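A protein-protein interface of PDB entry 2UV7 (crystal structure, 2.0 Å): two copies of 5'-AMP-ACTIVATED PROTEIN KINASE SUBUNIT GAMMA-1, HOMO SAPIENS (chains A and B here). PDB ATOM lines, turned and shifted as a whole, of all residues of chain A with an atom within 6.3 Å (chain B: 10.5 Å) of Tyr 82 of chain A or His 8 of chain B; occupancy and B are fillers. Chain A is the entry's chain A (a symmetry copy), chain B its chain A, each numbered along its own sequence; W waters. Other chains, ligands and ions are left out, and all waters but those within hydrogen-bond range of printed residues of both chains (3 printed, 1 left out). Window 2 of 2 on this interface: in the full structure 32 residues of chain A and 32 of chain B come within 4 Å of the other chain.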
ATOM      1  N   GLU A  79      10.651  15.154  18.274  1.00  0.00           N
ATOM      2  CA  GLU A  79      11.597  14.717  19.312  1.00  0.00           C
ATOM      3  C   GLU A  79      11.128  13.418  19.972  1.00  0.00           C
ATOM      4  O   GLU A  79       9.955  13.259  20.334  1.00  0.00           O
ATOM      5  CB  GLU A  79      11.810  15.803  20.367  1.00  0.00           C
ATOM      6  CG  GLU A  79      12.549  17.006  19.810  1.00  0.00           C
ATOM      7  CD  GLU A  79      12.817  18.093  20.819  1.00  0.00           C
ATOM      8  OE1 GLU A  79      12.727  17.806  22.024  1.00  0.00           O
ATOM      9  OE2 GLU A  79      13.125  19.241  20.392  1.00  0.00           O
ATOM     10  N   LYS A  80      12.047  12.482  20.112  1.00  0.00           N
ATOM     11  CA  LYS A  80      11.695  11.174  20.657  1.00  0.00           C
ATOM     12  C   LYS A  80      11.613  11.215  22.174  1.00  0.00           C
ATOM     13  O   LYS A  80      10.975  10.347  22.787  1.00  0.00           O
ATOM     14  CB  LYS A  80      12.666  10.100  20.162  1.00  0.00           C
ATOM     15  CG  LYS A  80      12.713  10.017  18.650  1.00  0.00           C
ATOM     16  CD  LYS A  80      12.643   8.591  18.120  1.00  0.00           C
ATOM     17  CE  LYS A  80      12.528   8.575  16.585  1.00  0.00           C
ATOM     18  NZ  LYS A  80      11.276   9.235  16.071  1.00  0.00           N
ATOM     19  N   THR A  81      12.221  12.228  22.789  1.00  0.00           N
ATOM     20  CA  THR A  81      12.080  12.389  24.231  1.00  0.00           C
ATOM     21  C   THR A  81      10.682  12.957  24.546  1.00  0.00           C
ATOM     22  O   THR A  81       9.997  13.495  23.651  1.00  0.00           O
ATOM     23  CB  THR A  81      13.209  13.263  24.798  1.00  0.00           C
ATOM     24  OG1 THR A  81      13.344  14.446  24.001  1.00  0.00           O
ATOM     25  CG2 THR A  81      14.523  12.506  24.779  1.00  0.00           C
ATOM     26  N   TYR A  82      10.252  12.813  25.795  1.00  0.00           N
ATOM     27  CA  TYR A  82       8.929  13.291  26.214  1.00  0.00           C
ATOM     28  C   TYR A  82       8.903  14.813  26.399  1.00  0.00           C
ATOM     29  O   TYR A  82       9.684  15.366  27.162  1.00  0.00           O
ATOM     30  CB  TYR A  82       8.479  12.566  27.493  1.00  0.00           C
ATOM     31  CG  TYR A  82       7.112  12.976  28.005  1.00  0.00           C
ATOM     32  CD1 TYR A  82       5.978  12.196  27.746  1.00  0.00           C
ATOM     33  CD2 TYR A  82       6.946  14.153  28.740  1.00  0.00           C
ATOM     34  CE1 TYR A  82       4.706  12.575  28.233  1.00  0.00           C
ATOM     35  CE2 TYR A  82       5.689  14.546  29.207  1.00  0.00           C
ATOM     36  CZ  TYR A  82       4.578  13.748  28.954  1.00  0.00           C
ATOM     37  OH  TYR A  82       3.346  14.143  29.424  1.00  0.00           O
ATOM     38  N   ASN A  83       7.994  15.488  25.688  1.00  0.00           N
ATOM     39  CA  ASN A  83       7.762  16.895  25.880  1.00  0.00           C
ATOM     40  C   ASN A  83       6.289  17.163  26.155  1.00  0.00           C
ATOM     41  O   ASN A  83       5.426  16.351  25.817  1.00  0.00           O
ATOM     42  CB  ASN A  83       8.208  17.711  24.654  1.00  0.00           C
ATOM     43  CG  ASN A  83       9.674  17.539  24.326  1.00  0.00           C
ATOM     44  OD1 ASN A  83      10.562  17.888  25.121  1.00  0.00           O
ATOM     45  ND2 ASN A  83       9.942  17.021  23.138  1.00  0.00           N
ATOM     46  N   ASN A  84       6.038  18.281  26.823  1.00  0.00           N
ATOM     47  CA  ASN A  84       4.727  18.920  26.839  1.00  0.00           C
ATOM     48  C   ASN A  84       4.834  20.353  26.254  1.00  0.00           C
ATOM     49  O   ASN A  84       5.921  20.818  25.925  1.00  0.00           O
ATOM     50  CB  ASN A  84       4.088  18.866  28.239  1.00  0.00           C
ATOM     51  CG  ASN A  84       4.930  19.541  29.322  1.00  0.00           C
ATOM     52  OD1 ASN A  84       5.365  20.685  29.176  1.00  0.00           O
ATOM     53  ND2 ASN A  84       5.147  18.829  30.419  1.00  0.00           N
ATOM     54  N   LEU A  85       3.711  21.047  26.094  1.00  0.00           N
ATOM     55  CA  LEU A  85       3.735  22.384  25.485  1.00  0.00           C
ATOM     56  C   LEU A  85       4.202  23.494  26.430  1.00  0.00           C
ATOM     57  O   LEU A  85       4.426  24.629  25.987  1.00  0.00           O
ATOM     58  CB  LEU A  85       2.354  22.751  24.927  1.00  0.00           C
ATOM     59  CG  LEU A  85       2.044  22.242  23.528  1.00  0.00           C
ATOM     60  CD1 LEU A  85       0.562  22.445  23.231  1.00  0.00           C
ATOM     61  CD2 LEU A  85       2.940  22.940  22.484  1.00  0.00           C
ATOM     62  N   ASP A  86       4.330  23.171  27.720  1.00  0.00           N
ATOM     63  CA  ASP A  86       4.907  24.091  28.688  1.00  0.00           C
ATOM     64  C   ASP A  86       6.434  24.235  28.526  1.00  0.00           C
ATOM     65  O   ASP A  86       7.065  24.972  29.258  1.00  0.00           O
ATOM     66  CB  ASP A  86       4.560  23.654  30.111  1.00  0.00           C
ATOM     67  CG  ASP A  86       4.603  24.805  31.117  1.00  0.00           C
ATOM     68  OD1 ASP A  86       4.705  26.001  30.734  1.00  0.00           O
ATOM     69  OD2 ASP A  86       4.546  24.495  32.317  1.00  0.00           O
ATOM     70  N   HIS B   8       0.780  17.002  30.204  1.00  0.00           N
ATOM     71  CA  HIS B   8      -0.205  17.311  29.104  1.00  0.00           C
ATOM     72  C   HIS B   8       0.332  17.022  27.701  1.00  0.00           C
ATOM     73  O   HIS B   8       1.364  17.569  27.265  1.00  0.00           O
ATOM     74  CB  HIS B   8      -0.626  18.763  29.216  1.00  0.00           C
ATOM     75  CG  HIS B   8       0.215  19.549  30.174  1.00  0.00           C
ATOM     76  ND1 HIS B   8       1.090  20.532  29.763  1.00  0.00           N
ATOM     77  CD2 HIS B   8       0.331  19.479  31.523  1.00  0.00           C
ATOM     78  CE1 HIS B   8       1.705  21.037  30.818  1.00  0.00           C
ATOM     79  NE2 HIS B   8       1.264  20.415  31.898  1.00  0.00           N
ATOM     80  N   GLU B   9       1.101  15.443  27.012  1.00  0.00           N
ATOM     81  CA  GLU B   9       2.222  15.218  26.137  1.00  0.00           C
ATOM     82  C   GLU B   9       2.042  16.002  24.822  1.00  0.00           C
ATOM     83  O   GLU B   9       0.921  16.122  24.307  1.00  0.00           O
ATOM     84  CB  GLU B   9       2.414  13.728  25.903  1.00  0.00           C
ATOM     85  CG  GLU B   9       3.737  13.449  25.227  1.00  0.00           C
ATOM     86  CD  GLU B   9       3.993  12.001  24.909  1.00  0.00           C
ATOM     87  OE1 GLU B   9       4.969  11.755  24.176  1.00  0.00           O
ATOM     88  OE2 GLU B   9       3.256  11.124  25.394  1.00  0.00           O
ATOM     89  N   PHE B  10       3.137  16.597  24.340  1.00  0.00           N
ATOM     90  CA  PHE B  10       3.208  17.198  23.019  1.00  0.00           C
ATOM     91  C   PHE B  10       4.217  16.454  22.130  1.00  0.00           C
ATOM     92  O   PHE B  10       5.377  16.301  22.493  1.00  0.00           O
ATOM     93  CB  PHE B  10       3.562  18.690  23.053  1.00  0.00           C
ATOM     94  CG  PHE B  10       3.535  19.324  21.689  1.00  0.00           C
ATOM     95  CD1 PHE B  10       2.316  19.693  21.103  1.00  0.00           C
ATOM     96  CD2 PHE B  10       4.696  19.470  20.951  1.00  0.00           C
ATOM     97  CE1 PHE B  10       2.276  20.249  19.818  1.00  0.00           C
ATOM     98  CE2 PHE B  10       4.667  19.997  19.669  1.00  0.00           C
ATOM     99  CZ  PHE B  10       3.450  20.410  19.105  1.00  0.00           C
ATOM    100  N   PRO B  11       3.764  15.958  20.971  1.00  0.00           N
ATOM    101  CA  PRO B  11       2.397  15.967  20.500  1.00  0.00           C
ATOM    102  C   PRO B  11       1.549  14.862  21.185  1.00  0.00           C
ATOM    103  O   PRO B  11       2.111  13.934  21.785  1.00  0.00           O
ATOM    104  CB  PRO B  11       2.558  15.751  18.998  1.00  0.00           C
ATOM    105  CG  PRO B  11       3.804  14.994  18.852  1.00  0.00           C
ATOM    106  CD  PRO B  11       4.661  15.272  20.032  1.00  0.00           C
ATOM    107  N   LYS B  12       0.214  14.979  21.130  1.00  0.00           N
ATOM    108  CA  LYS B  12      -0.667  13.947  21.704  1.00  0.00           C
ATOM    109  C   LYS B  12      -0.492  12.619  20.987  1.00  0.00           C
ATOM    110  O   LYS B  12      -0.635  12.545  19.766  1.00  0.00           O
ATOM    111  CB  LYS B  12      -2.137  14.359  21.633  1.00  0.00           C
ATOM    112  CG  LYS B  12      -2.508  15.485  22.571  1.00  0.00           C
ATOM    113  CD  LYS B  12      -4.017  15.725  22.624  1.00  0.00           C
ATOM    114  CE  LYS B  12      -4.431  16.171  24.025  1.00  0.00           C
ATOM    115  NZ  LYS B  12      -4.525  15.024  24.991  1.00  0.00           N
ATOM    116  N   PRO B  13      -0.196  11.544  21.735  1.00  0.00           N
ATOM    117  CA  PRO B  13       0.029  10.248  21.070  1.00  0.00           C
ATOM    118  C   PRO B  13      -1.178   9.678  20.284  1.00  0.00           C
ATOM    119  O   PRO B  13      -1.003   8.996  19.261  1.00  0.00           O
ATOM    120  CB  PRO B  13       0.398   9.309  22.239  1.00  0.00           C
ATOM    121  CG  PRO B  13       0.765  10.209  23.365  1.00  0.00           C
ATOM    122  CD  PRO B  13      -0.047  11.449  23.200  1.00  0.00           C
ATOM    123  N   GLU B  14      -2.378   9.974  20.766  1.00  0.00           N
ATOM    124  CA  GLU B  14      -3.613   9.557  20.122  1.00  0.00           C
ATOM    125  C   GLU B  14      -3.862  10.246  18.771  1.00  0.00           C
ATOM    126  O   GLU B  14      -4.568   9.700  17.924  1.00  0.00           O
ATOM    127  CB  GLU B  14      -4.819   9.755  21.066  1.00  0.00           C
ATOM    128  CG  GLU B  14      -5.090  11.201  21.517  1.00  0.00           C
ATOM    129  CD  GLU B  14      -4.584  11.534  22.939  1.00  0.00           C
ATOM    130  OE1 GLU B  14      -5.248  12.382  23.595  1.00  0.00           O
ATOM    131  OE2 GLU B  14      -3.532  10.988  23.381  1.00  0.00           O
ATOM    132  N   LEU B 149      -1.920  19.663  15.163  1.00  0.00           N
ATOM    133  CA  LEU B 149      -1.189  19.609  16.439  1.00  0.00           C
ATOM    134  C   LEU B 149      -1.956  20.339  17.556  1.00  0.00           C
ATOM    135  O   LEU B 149      -1.627  20.172  18.722  1.00  0.00           O
ATOM    136  CB  LEU B 149       0.258  20.124  16.290  1.00  0.00           C
ATOM    137  CG  LEU B 149       1.257  19.210  15.552  1.00  0.00           C
ATOM    138  CD1 LEU B 149       2.601  19.866  15.306  1.00  0.00           C
ATOM    139  CD2 LEU B 149       1.443  17.863  16.257  1.00  0.00           C
HETATM  140  O   HOH W   1       7.899  16.038  21.404  1.00  0.00           O
HETATM  141  O   HOH W   2       3.305  16.408  30.833  1.00  0.00           O
HETATM  142  O   HOH W   3       1.042  19.850  25.938  1.00  0.00           O
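The backbone NH (N) of Phe 10 of chain B is in hydrogen-bond range of the backbone carbonyl oxygen (O) of Asn 83 of chain A (2.7 Å).
Water W3 bridges the backbone carbonyl oxygen of His 8 of chain B (2.7 Å) and the backbone NH of Leu 85 of chain A (2.9 Å).
Water W2 lies within hydrogen-bond range of the side-chain hydroxyl of Tyr 82 of chain A (2.7 Å), the backbone NH of His 8 of chain B (2.7 Å) and the side-chain amide nitrogen of Asn 84 of chain A (3.1 Å).
Water W1 lies within hydrogen-bond range of O of Phe 10 of chain B (2.8 Å) and ND2 of Asn 83 of chain A (2.9 Å).
Tyr 82 of chain A touches His 8 of chain B (OH to N, 3.9 Å).
CG of Glu 9 of chain B touches CE1 of Tyr 82 of chain A, at 3.3 Å.
O of Asn 83 of chain A touches CG of Glu 9 of chain B, 3.4 Å away.
CB of Asn 84 of chain A touches O of His 8 of chain B, at 3.2 Å.
Phe 10 of chain B touches Asn 84 of chain A.
CG of Leu 85 of chain A touches CD1 of Phe 10 of chain B, at 3.5 Å.
His 8 of chain B touches Asp 86 of chain A.
Printed residues of chain B that touch a printed residue of chain A: His 8, Glu 9 and Phe 10.
Hydrophobic or aromatic side chains of chain A that line the printed part of chain B: Tyr 82 and Leu 85.
Among the printed residues, 8 pairs touch across the chains.
No position is printed for both chains.
Of the 8 pairs that touch across the chains among the printed residues, none has its exchanged pair printed and touching as well.
The side-chain carboxylate (OE1) of Glu 79 of chain A is in hydrogen-bond range of the side-chain amide nitrogen (ND2) of Asn 83 of chain A.
The side-chain amide oxygen (OD1) of Asn 84 of chain A lies within hydrogen-bond range of the backbone NH (N) of Asp 86 of chain A (3.1 Å).
Printed residues of chain B within 4 Å of Tyr 82 of chain A: His 8 and Glu 9.
Of chain A, only Tyr 82 (3.9 Å), Asn 84 (3.2 Å) and Asp 86 (3.9 Å) come within 4 Å of His 8 of chain B.
No residue of chain B comes within 4 Å of Thr 81 of chain A.
Asn 84 of chain A touches just these residues of chain B: His 8 (3.2 Å) and Phe 10 (3.8 Å).
Printed residues of chain B within 4 Å of Leu 85 of chain A: Phe 10 (3.5 Å).
Of the printed residues of chain A, Phe 10 of chain B touches Asn 83, Asn 84 and Leu 85.
Of the printed residues of chain B, Asp 86 of chain A touches His 8.
Of the printed residues of chain A, Glu 9 of chain B touches Tyr 82 and Asn 83.
Glu 79 of chain A touches none of the printed residues of chain B.
Lys 80 of chain A touches none of the printed residues of chain B.
The nearest printed residue of chain A that does not touch Phe 10 of chain B is Tyr 82 of chain A (5.5 Å).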
